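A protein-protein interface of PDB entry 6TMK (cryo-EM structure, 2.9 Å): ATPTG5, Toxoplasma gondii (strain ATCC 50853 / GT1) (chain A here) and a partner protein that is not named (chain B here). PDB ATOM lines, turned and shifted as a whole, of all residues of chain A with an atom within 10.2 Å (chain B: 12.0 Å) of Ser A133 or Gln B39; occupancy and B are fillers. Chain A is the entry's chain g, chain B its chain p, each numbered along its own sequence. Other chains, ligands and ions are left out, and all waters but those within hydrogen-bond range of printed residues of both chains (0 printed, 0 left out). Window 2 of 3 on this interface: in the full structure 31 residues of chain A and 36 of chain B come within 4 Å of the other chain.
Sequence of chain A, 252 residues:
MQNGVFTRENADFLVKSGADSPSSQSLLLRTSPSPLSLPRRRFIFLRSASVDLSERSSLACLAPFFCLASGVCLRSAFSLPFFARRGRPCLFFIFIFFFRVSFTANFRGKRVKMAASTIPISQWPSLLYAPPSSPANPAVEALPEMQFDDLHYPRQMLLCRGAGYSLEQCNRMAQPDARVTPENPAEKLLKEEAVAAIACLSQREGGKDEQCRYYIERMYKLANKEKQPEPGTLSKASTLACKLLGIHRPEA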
ATOM      1  N   ALA A 115      20.215  16.810   6.599  1.00  0.00           N
ATOM      2  CA  ALA A 115      19.550  16.741   5.305  1.00  0.00           C
ATOM      3  C   ALA A 115      18.372  15.780   5.363  1.00  0.00           C
ATOM      4  O   ALA A 115      17.251  16.135   5.001  1.00  0.00           O
ATOM      5  CB  ALA A 115      20.529  16.314   4.225  1.00  0.00           C
ATOM      6  N   ALA A 116      18.632  14.556   5.818  1.00  0.00           N
ATOM      7  CA  ALA A 116      17.577  13.571   6.030  1.00  0.00           C
ATOM      8  C   ALA A 116      16.847  13.925   7.315  1.00  0.00           C
ATOM      9  O   ALA A 116      17.305  13.611   8.414  1.00  0.00           O
ATOM     10  CB  ALA A 116      18.157  12.166   6.094  1.00  0.00           C
ATOM     11  N   ILE A 119      10.732  11.967   9.798  1.00  0.00           N
ATOM     12  CA  ILE A 119       9.410  11.754   9.219  1.00  0.00           C
ATOM     13  C   ILE A 119       8.433  11.572  10.377  1.00  0.00           C
ATOM     14  O   ILE A 119       8.544  10.577  11.110  1.00  0.00           O
ATOM     15  CB  ILE A 119       9.386  10.537   8.287  1.00  0.00           C
ATOM     16  CG1 ILE A 119      10.596  10.530   7.358  1.00  0.00           C
ATOM     17  CG2 ILE A 119       8.107  10.518   7.479  1.00  0.00           C
ATOM     18  CD1 ILE A 119      10.780  11.778   6.585  1.00  0.00           C
ATOM     19  N   LEU A 127       5.297   6.983   3.540  1.00  0.00           N
ATOM     20  CA  LEU A 127       6.647   6.449   3.590  1.00  0.00           C
ATOM     21  C   LEU A 127       6.680   4.974   3.227  1.00  0.00           C
ATOM     22  O   LEU A 127       7.689   4.485   2.711  1.00  0.00           O
ATOM     23  CB  LEU A 127       7.216   6.667   4.985  1.00  0.00           C
ATOM     24  CG  LEU A 127       8.549   6.037   5.352  1.00  0.00           C
ATOM     25  CD1 LEU A 127       9.633   6.553   4.459  1.00  0.00           C
ATOM     26  CD2 LEU A 127       8.842   6.345   6.789  1.00  0.00           C
ATOM     27  N   ALA A 130       6.111   5.066  -0.739  1.00  0.00           N
ATOM     28  CA  ALA A 130       7.025   5.951  -1.459  1.00  0.00           C
ATOM     29  C   ALA A 130       8.247   6.193  -0.588  1.00  0.00           C
ATOM     30  O   ALA A 130       8.488   7.309  -0.118  1.00  0.00           O
ATOM     31  CB  ALA A 130       6.341   7.268  -1.824  1.00  0.00           C
ATOM     32  N   PRO A 131       9.044   5.160  -0.349  1.00  0.00           N
ATOM     33  CA  PRO A 131      10.159   5.291   0.580  1.00  0.00           C
ATOM     34  C   PRO A 131      11.253   6.165  -0.001  1.00  0.00           C
ATOM     35  O   PRO A 131      11.295   6.399  -1.217  1.00  0.00           O
ATOM     36  CB  PRO A 131      10.640   3.848   0.763  1.00  0.00           C
ATOM     37  CG  PRO A 131      10.191   3.144  -0.436  1.00  0.00           C
ATOM     38  CD  PRO A 131       8.946   3.803  -0.906  1.00  0.00           C
ATOM     39  N   PRO A 132      12.155   6.667   0.834  1.00  0.00           N
ATOM     40  CA  PRO A 132      13.254   7.485   0.324  1.00  0.00           C
ATOM     41  C   PRO A 132      14.239   6.655  -0.481  1.00  0.00           C
ATOM     42  O   PRO A 132      14.190   5.425  -0.516  1.00  0.00           O
ATOM     43  CB  PRO A 132      13.894   8.038   1.597  1.00  0.00           C
ATOM     44  CG  PRO A 132      13.559   7.040   2.629  1.00  0.00           C
ATOM     45  CD  PRO A 132      12.190   6.577   2.300  1.00  0.00           C
ATOM     46  N   SER A 133      15.155   7.362  -1.134  1.00  0.00           N
ATOM     47  CA  SER A 133      16.125   6.719  -2.003  1.00  0.00           C
ATOM     48  C   SER A 133      17.226   6.055  -1.192  1.00  0.00           C
ATOM     49  O   SER A 133      17.660   6.570  -0.159  1.00  0.00           O
ATOM     50  CB  SER A 133      16.723   7.734  -2.973  1.00  0.00           C
ATOM     51  OG  SER A 133      15.717   8.287  -3.802  1.00  0.00           O
ATOM     52  N   SER A 134      17.671   4.907  -1.674  1.00  0.00           N
ATOM     53  CA  SER A 134      18.722   4.132  -1.038  1.00  0.00           C
ATOM     54  C   SER A 134      19.665   3.609  -2.111  1.00  0.00           C
ATOM     55  O   SER A 134      19.347   3.674  -3.305  1.00  0.00           O
ATOM     56  CB  SER A 134      18.139   2.978  -0.226  1.00  0.00           C
ATOM     57  OG  SER A 134      17.349   3.450   0.845  1.00  0.00           O
ATOM     58  N   PRO A 135      20.832   3.089  -1.731  1.00  0.00           N
ATOM     59  CA  PRO A 135      21.634   2.329  -2.697  1.00  0.00           C
ATOM     60  C   PRO A 135      21.002   1.012  -3.088  1.00  0.00           C
ATOM     61  O   PRO A 135      21.366   0.456  -4.132  1.00  0.00           O
ATOM     62  CB  PRO A 135      22.961   2.111  -1.963  1.00  0.00           C
ATOM     63  CG  PRO A 135      22.953   3.049  -0.821  1.00  0.00           C
ATOM     64  CD  PRO A 135      21.541   3.301  -0.465  1.00  0.00           C
ATOM     65  N   ALA A 136      20.070   0.495  -2.291  1.00  0.00           N
ATOM     66  CA  ALA A 136      19.344  -0.733  -2.594  1.00  0.00           C
ATOM     67  C   ALA A 136      17.862  -0.428  -2.421  1.00  0.00           C
ATOM     68  O   ALA A 136      17.288  -0.672  -1.357  1.00  0.00           O
ATOM     69  CB  ALA A 136      19.793  -1.876  -1.701  1.00  0.00           C
ATOM     70  N   ASN A 137      17.251   0.102  -3.464  1.00  0.00           N
ATOM     71  CA  ASN A 137      15.843   0.446  -3.430  1.00  0.00           C
ATOM     72  C   ASN A 137      14.987  -0.753  -3.803  1.00  0.00           C
ATOM     73  O   ASN A 137      15.461  -1.698  -4.441  1.00  0.00           O
ATOM     74  CB  ASN A 137      15.558   1.594  -4.390  1.00  0.00           C
ATOM     75  CG  ASN A 137      16.261   2.871  -3.996  1.00  0.00           C
ATOM     76  OD1 ASN A 137      15.873   3.536  -3.037  1.00  0.00           O
ATOM     77  ND2 ASN A 137      17.299   3.225  -4.739  1.00  0.00           N
ATOM     78  N   PRO A 138      13.720  -0.748  -3.411  1.00  0.00           N
ATOM     79  CA  PRO A 138      12.775  -1.715  -3.973  1.00  0.00           C
ATOM     80  C   PRO A 138      12.058  -1.175  -5.196  1.00  0.00           C
ATOM     81  O   PRO A 138      12.279  -0.031  -5.603  1.00  0.00           O
ATOM     82  CB  PRO A 138      11.808  -1.951  -2.814  1.00  0.00           C
ATOM     83  CG  PRO A 138      11.764  -0.634  -2.133  1.00  0.00           C
ATOM     84  CD  PRO A 138      13.124  -0.008  -2.289  1.00  0.00           C
ATOM     85  N   VAL A 140       9.162   0.462  -6.263  1.00  0.00           N
ATOM     86  CA  VAL A 140       8.062   1.221  -5.679  1.00  0.00           C
ATOM     87  C   VAL A 140       6.778   1.010  -6.470  1.00  0.00           C
ATOM     88  O   VAL A 140       5.680   0.978  -5.903  1.00  0.00           O
ATOM     89  CB  VAL A 140       8.434   2.710  -5.595  1.00  0.00           C
ATOM     90  CG1 VAL A 140       9.628   2.894  -4.698  1.00  0.00           C
ATOM     91  CG2 VAL A 140       8.721   3.266  -6.976  1.00  0.00           C
ATOM     92  N   ALA B  30      20.015  -9.493   5.732  1.00  0.00           N
ATOM     93  CA  ALA B  30      19.624  -8.465   6.687  1.00  0.00           C
ATOM     94  C   ALA B  30      20.681  -7.374   6.796  1.00  0.00           C
ATOM     95  O   ALA B  30      20.354  -6.183   6.873  1.00  0.00           O
ATOM     96  CB  ALA B  30      19.366  -9.101   8.049  1.00  0.00           C
ATOM     97  N   ALA B  31      21.956  -7.763   6.799  1.00  0.00           N
ATOM     98  CA  ALA B  31      23.031  -6.783   6.889  1.00  0.00           C
ATOM     99  C   ALA B  31      23.066  -5.883   5.664  1.00  0.00           C
ATOM    100  O   ALA B  31      23.289  -4.675   5.779  1.00  0.00           O
ATOM    101  CB  ALA B  31      24.367  -7.493   7.068  1.00  0.00           C
ATOM    102  N   TYR B  32      22.868  -6.460   4.481  1.00  0.00           N
ATOM    103  CA  TYR B  32      22.818  -5.667   3.261  1.00  0.00           C
ATOM    104  C   TYR B  32      21.707  -4.632   3.334  1.00  0.00           C
ATOM    105  O   TYR B  32      21.909  -3.458   3.001  1.00  0.00           O
ATOM    106  CB  TYR B  32      22.628  -6.587   2.059  1.00  0.00           C
ATOM    107  CG  TYR B  32      22.942  -5.955   0.730  1.00  0.00           C
ATOM    108  CD1 TYR B  32      24.222  -5.987   0.210  1.00  0.00           C
ATOM    109  CD2 TYR B  32      21.951  -5.349  -0.019  1.00  0.00           C
ATOM    110  CE1 TYR B  32      24.508  -5.417  -1.006  1.00  0.00           C
ATOM    111  CE2 TYR B  32      22.229  -4.778  -1.233  1.00  0.00           C
ATOM    112  CZ  TYR B  32      23.507  -4.817  -1.725  1.00  0.00           C
ATOM    113  OH  TYR B  32      23.788  -4.248  -2.943  1.00  0.00           O
ATOM    114  N   ASP B  33      20.522  -5.049   3.779  1.00  0.00           N
ATOM    115  CA  ASP B  33      19.407  -4.113   3.879  1.00  0.00           C
ATOM    116  C   ASP B  33      19.696  -3.002   4.886  1.00  0.00           C
ATOM    117  O   ASP B  33      19.426  -1.821   4.618  1.00  0.00           O
ATOM    118  CB  ASP B  33      18.137  -4.870   4.249  1.00  0.00           C
ATOM    119  CG  ASP B  33      17.665  -5.789   3.141  1.00  0.00           C
ATOM    120  OD1 ASP B  33      17.639  -7.018   3.356  1.00  0.00           O
ATOM    121  OD2 ASP B  33      17.327  -5.284   2.050  1.00  0.00           O
ATOM    122  N   SER B  34      20.249  -3.355   6.046  1.00  0.00           N
ATOM    123  CA  SER B  34      20.554  -2.343   7.053  1.00  0.00           C
ATOM    124  C   SER B  34      21.593  -1.354   6.542  1.00  0.00           C
ATOM    125  O   SER B  34      21.452  -0.139   6.728  1.00  0.00           O
ATOM    126  CB  SER B  34      21.041  -3.010   8.337  1.00  0.00           C
ATOM    127  OG  SER B  34      20.143  -4.013   8.772  1.00  0.00           O
ATOM    128  N   ALA B  35      22.649  -1.855   5.907  1.00  0.00           N
ATOM    129  CA  ALA B  35      23.687  -0.981   5.380  1.00  0.00           C
ATOM    130  C   ALA B  35      23.160  -0.099   4.262  1.00  0.00           C
ATOM    131  O   ALA B  35      23.617   1.035   4.109  1.00  0.00           O
ATOM    132  CB  ALA B  35      24.867  -1.809   4.892  1.00  0.00           C
ATOM    133  N   ALA B  36      22.214  -0.594   3.468  1.00  0.00           N
ATOM    134  CA  ALA B  36      21.591   0.257   2.465  1.00  0.00           C
ATOM    135  C   ALA B  36      20.804   1.378   3.120  1.00  0.00           C
ATOM    136  O   ALA B  36      20.883   2.535   2.692  1.00  0.00           O
ATOM    137  CB  ALA B  36      20.682  -0.570   1.568  1.00  0.00           C
ATOM    138  N   GLY B  37      20.036   1.056   4.157  1.00  0.00           N
ATOM    139  CA  GLY B  37      19.300   2.092   4.857  1.00  0.00           C
ATOM    140  C   GLY B  37      20.206   3.133   5.483  1.00  0.00           C
ATOM    141  O   GLY B  37      19.880   4.321   5.508  1.00  0.00           O
ATOM    142  N   TRP B  38      21.355   2.704   5.994  1.00  0.00           N
ATOM    143  CA  TRP B  38      22.308   3.592   6.650  1.00  0.00           C
ATOM    144  C   TRP B  38      23.372   4.144   5.708  1.00  0.00           C
ATOM    145  O   TRP B  38      24.282   4.839   6.168  1.00  0.00           O
ATOM    146  CB  TRP B  38      22.989   2.866   7.804  1.00  0.00           C
ATOM    147  CG  TRP B  38      22.108   2.644   8.974  1.00  0.00           C
ATOM    148  CD1 TRP B  38      21.505   1.482   9.327  1.00  0.00           C
ATOM    149  CD2 TRP B  38      21.727   3.608   9.955  1.00  0.00           C
ATOM    150  NE1 TRP B  38      20.773   1.656  10.466  1.00  0.00           N
ATOM    151  CE2 TRP B  38      20.893   2.957  10.872  1.00  0.00           C
ATOM    152  CE3 TRP B  38      22.013   4.959  10.148  1.00  0.00           C
ATOM    153  CZ2 TRP B  38      20.340   3.607  11.963  1.00  0.00           C
ATOM    154  CZ3 TRP B  38      21.461   5.599  11.228  1.00  0.00           C
ATOM    155  CH2 TRP B  38      20.638   4.926  12.121  1.00  0.00           C
ATOM    156  N   GLN B  39      23.276   3.865   4.410  1.00  0.00           N
ATOM    157  CA  GLN B  39      24.166   4.440   3.404  1.00  0.00           C
ATOM    158  C   GLN B  39      25.623   4.020   3.625  1.00  0.00           C
ATOM    159  O   GLN B  39      26.505   4.847   3.861  1.00  0.00           O
ATOM    160  CB  GLN B  39      24.052   5.966   3.414  1.00  0.00           C
ATOM    161  CG  GLN B  39      22.643   6.535   3.344  1.00  0.00           C
ATOM    162  CD  GLN B  39      22.060   6.535   1.953  1.00  0.00           C
ATOM    163  OE1 GLN B  39      22.759   6.785   0.973  1.00  0.00           O
ATOM    164  NE2 GLN B  39      20.763   6.286   1.862  1.00  0.00           N
ATOM    165  N   GLU B  40      25.869   2.710   3.539  1.00  0.00           N
ATOM    166  CA  GLU B  40      27.182   2.134   3.839  1.00  0.00           C
ATOM    167  C   GLU B  40      27.633   1.189   2.731  1.00  0.00           C
ATOM    168  O   GLU B  40      27.447  -0.038   2.819  1.00  0.00           O
ATOM    169  CB  GLU B  40      27.164   1.428   5.187  1.00  0.00           C
ATOM    170  CG  GLU B  40      26.869   2.359   6.329  1.00  0.00           C
ATOM    171  CD  GLU B  40      27.999   3.328   6.606  1.00  0.00           C
ATOM    172  OE1 GLU B  40      29.099   3.137   6.048  1.00  0.00           O
ATOM    173  OE2 GLU B  40      27.785   4.285   7.378  1.00  0.00           O
ATOM    174  N   PRO B  41      28.267   1.723   1.681  1.00  0.00           N
ATOM    175  CA  PRO B  41      28.714   0.859   0.579  1.00  0.00           C
ATOM    176  C   PRO B  41      29.754  -0.163   0.990  1.00  0.00           C
ATOM    177  O   PRO B  41      29.726  -1.298   0.504  1.00  0.00           O
ATOM    178  CB  PRO B  41      29.271   1.865  -0.438  1.00  0.00           C
ATOM    179  CG  PRO B  41      29.592   3.068   0.361  1.00  0.00           C
ATOM    180  CD  PRO B  41      28.538   3.138   1.395  1.00  0.00           C
ATOM    181  N   LYS B  42      30.670   0.204   1.884  1.00  0.00           N
ATOM    182  CA  LYS B  42      31.704  -0.728   2.316  1.00  0.00           C
ATOM    183  C   LYS B  42      31.085  -1.942   2.995  1.00  0.00           C
ATOM    184  O   LYS B  42      31.396  -3.094   2.662  1.00  0.00           O
ATOM    185  CB  LYS B  42      32.674  -0.012   3.251  1.00  0.00           C
ATOM    186  CG  LYS B  42      33.606  -0.922   4.019  1.00  0.00           C
ATOM    187  CD  LYS B  42      34.751  -0.140   4.641  1.00  0.00           C
ATOM    188  CE  LYS B  42      34.238   1.059   5.428  1.00  0.00           C
ATOM    189  NZ  LYS B  42      35.214   1.559   6.428  1.00  0.00           N
ATOM    190  N   ALA B  43      30.178  -1.695   3.938  1.00  0.00           N
ATOM    191  CA  ALA B  43      29.538  -2.785   4.659  1.00  0.00           C
ATOM    192  C   ALA B  43      28.701  -3.642   3.725  1.00  0.00           C
ATOM    193  O   ALA B  43      28.733  -4.878   3.809  1.00  0.00           O
ATOM    194  CB  ALA B  43      28.675  -2.227   5.783  1.00  0.00           C
ATOM    195  N   MET B  44      27.946  -3.017   2.823  1.00  0.00           N
ATOM    196  CA  MET B  44      27.066  -3.821   1.988  1.00  0.00           C
ATOM    197  C   MET B  44      27.841  -4.593   0.925  1.00  0.00           C
ATOM    198  O   MET B  44      27.432  -5.698   0.549  1.00  0.00           O
ATOM    199  CB  MET B  44      25.998  -2.931   1.365  1.00  0.00           C
ATOM    200  CG  MET B  44      26.510  -1.915   0.405  1.00  0.00           C
ATOM    201  SD  MET B  44      25.471  -0.446   0.470  1.00  0.00           S
ATOM    202  CE  MET B  44      23.937  -1.120  -0.121  1.00  0.00           C
ATOM    203  N   GLU B  45      28.988  -4.081   0.475  1.00  0.00           N
ATOM    204  CA  GLU B  45      29.807  -4.864  -0.443  1.00  0.00           C
ATOM    205  C   GLU B  45      30.486  -6.015   0.285  1.00  0.00           C
ATOM    206  O   GLU B  45      30.641  -7.105  -0.277  1.00  0.00           O
ATOM    207  CB  GLU B  45      30.841  -3.978  -1.136  1.00  0.00           C
ATOM    208  CG  GLU B  45      31.947  -3.469  -0.242  1.00  0.00           C
ATOM    209  CD  GLU B  45      33.047  -2.769  -1.015  1.00  0.00           C
ATOM    210  OE1 GLU B  45      33.252  -3.106  -2.199  1.00  0.00           O
ATOM    211  OE2 GLU B  45      33.712  -1.883  -0.436  1.00  0.00           O
ATOM    212  N   SER B  46      30.890  -5.801   1.540  1.00  0.00           N
ATOM    213  CA  SER B  46      31.389  -6.913   2.341  1.00  0.00           C
ATOM    214  C   SER B  46      30.331  -7.998   2.472  1.00  0.00           C
ATOM    215  O   SER B  46      30.626  -9.195   2.340  1.00  0.00           O
ATOM    216  CB  SER B  46      31.812  -6.412   3.716  1.00  0.00           C
ATOM    217  OG  SER B  46      32.746  -5.355   3.604  1.00  0.00           O
ATOM    218  N   ALA B  47      29.092  -7.592   2.741  1.00  0.00           N
ATOM    219  CA  ALA B  47      27.999  -8.548   2.845  1.00  0.00           C
ATOM    220  C   ALA B  47      27.810  -9.312   1.544  1.00  0.00           C
ATOM    221  O   ALA B  47      27.634 -10.535   1.552  1.00  0.00           O
ATOM    222  CB  ALA B  47      26.715  -7.822   3.228  1.00  0.00           C
ATOM    223  N   ARG B  86       9.753  -8.603  -0.057  1.00  0.00           N
ATOM    224  CA  ARG B  86       9.916  -7.322  -0.715  1.00  0.00           C
ATOM    225  C   ARG B  86      10.367  -7.536  -2.156  1.00  0.00           C
ATOM    226  O   ARG B  86      11.262  -8.347  -2.410  1.00  0.00           O
ATOM    227  CB  ARG B  86      10.935  -6.473   0.028  1.00  0.00           C
ATOM    228  CG  ARG B  86      10.755  -4.991  -0.138  1.00  0.00           C
ATOM    229  CD  ARG B  86      11.822  -4.240   0.613  1.00  0.00           C
ATOM    230  NE  ARG B  86      11.606  -4.284   2.055  1.00  0.00           N
ATOM    231  CZ  ARG B  86      12.337  -3.613   2.938  1.00  0.00           C
ATOM    232  NH1 ARG B  86      13.335  -2.841   2.532  1.00  0.00           N
ATOM    233  NH2 ARG B  86      12.063  -3.714   4.229  1.00  0.00           N
ATOM    234  N   ASP B  89      14.488  -4.247  -6.788  1.00  0.00           N
ATOM    235  CA  ASP B  89      14.491  -3.428  -7.988  1.00  0.00           C
ATOM    236  C   ASP B  89      15.003  -4.245  -9.165  1.00  0.00           C
ATOM    237  O   ASP B  89      16.065  -4.869  -9.089  1.00  0.00           O
ATOM    238  CB  ASP B  89      15.355  -2.186  -7.782  1.00  0.00           C
ATOM    239  CG  ASP B  89      15.073  -1.103  -8.799  1.00  0.00           C
ATOM    240  OD1 ASP B  89      14.112  -1.250  -9.581  1.00  0.00           O
ATOM    241  OD2 ASP B  89      15.813  -0.097  -8.812  1.00  0.00           O
ATOM    242  N   ASP B  92      18.796  -3.580 -10.217  1.00  0.00           N
ATOM    243  CA  ASP B  92      19.983  -3.726  -9.390  1.00  0.00           C
ATOM    244  C   ASP B  92      20.486  -5.159  -9.434  1.00  0.00           C
ATOM    245  O   ASP B  92      19.878  -6.050  -8.805  1.00  0.00           O
ATOM    246  CB  ASP B  92      19.701  -3.306  -7.951  1.00  0.00           C
ATOM    247  CG  ASP B  92      19.076  -1.934  -7.859  1.00  0.00           C
ATOM    248  OD1 ASP B  92      18.322  -1.680  -6.896  1.00  0.00           O
ATOM    249  OD2 ASP B  92      19.340  -1.105  -8.755  1.00  0.00           O
ATOM    250  N   GLN B  95      21.217  -7.226  -6.017  1.00  0.00           N
ATOM    251  CA  GLN B  95      19.988  -7.718  -5.409  1.00  0.00           C
ATOM    252  C   GLN B  95      19.425  -8.891  -6.197  1.00  0.00           C
ATOM    253  O   GLN B  95      19.034  -9.917  -5.622  1.00  0.00           O
ATOM    254  CB  GLN B  95      18.973  -6.585  -5.335  1.00  0.00           C
ATOM    255  CG  GLN B  95      19.234  -5.593  -4.230  1.00  0.00           C
ATOM    256  CD  GLN B  95      18.292  -4.412  -4.283  1.00  0.00           C
ATOM    257  OE1 GLN B  95      18.468  -3.502  -5.087  1.00  0.00           O
ATOM    258  NE2 GLN B  95      17.286  -4.420  -3.424  1.00  0.00           N
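Among the printed residues, merely in contact across the chains: Pro A135 with Ala B36 (3.3 Å), Asn A137 with Asp B89 (3.4 Å), Ala A136 with Ala B36 (3.6 Å), Ser A133 with Gln B39 (3.7 Å), Asn A137 with Asp B92 (3.8 Å), Ala A136 with Tyr B32 (3.8 Å), Ala A136 with Gln B95 (3.8 Å), Pro A135 with Met B44 (3.8 Å) and Pro A135 with Gln B39 (3.9 Å).
The side-chain amide nitrogen of Gln B95 lies within hydrogen-bond range of the backbone carbonyl oxygen of Asn A137.
The backbone carbonyl oxygen (O) of Ser A134 is in hydrogen-bond range of the side-chain amide nitrogen (ND2) of Asn A137 (2.5 Å). The side-chain carboxylate of Asp B92 sits close to the side-chain amide oxygen of Gln B95 (2.6 Å).
Of the 22 printed residues of chain B, 7 touch a printed residue of chain A. Printed residues of chain B that touch a printed residue of chain A: Tyr B32, Ala B36, Gln B39, Met B44, Asp B89, Asp B92 and Gln B95. Of the 14 printed residues of chain A, 4 touch a printed residue of chain B. Printed residues of chain A that touch a printed residue of chain B: Ser A133, Pro A135, Ala A136 and Asn A137. Hydrophobic or aromatic side chains of chain A that line the printed part of chain B: Pro A135 and Ala A136. Among the printed residues, no Asp or Glu carboxylate lies within 4 Å of a Lys or Arg side-chain nitrogen of the other chain.
Leu A127 touches none of the printed residues of chain B. Pro A131 touches none of the printed residues of chain B. Of chain B, only Gln B39 comes within 4 Å of Ser A133. No residue of chain B comes within 4 Å of Ser A134. Of chain B, only Ala B36 (3.3 Å), Gln B39 (3.9 Å) and Met B44 (3.8 Å) come within 4 Å of Pro A135. Printed residues of chain A within 4 Å of Tyr B32: Ala A136. Printed residues of chain A within 4 Å of Ala B36: Pro A135 and Ala A136. No residue of chain A comes within 4 Å of Gly B37. No residue of chain A comes within 4 Å of Glu B40. Of the printed residues of chain A, Asp B92 touches Asn A137. The nearest residue of chain B that does not touch Ser A133 is Ala B36 (5.9 Å). The nearest residue of chain A that does not touch Gln B39 is Ser A134 (4.1 Å). The nearest printed residue of chain A that does not touch Tyr B32 is Pro A135 (5.4 Å).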
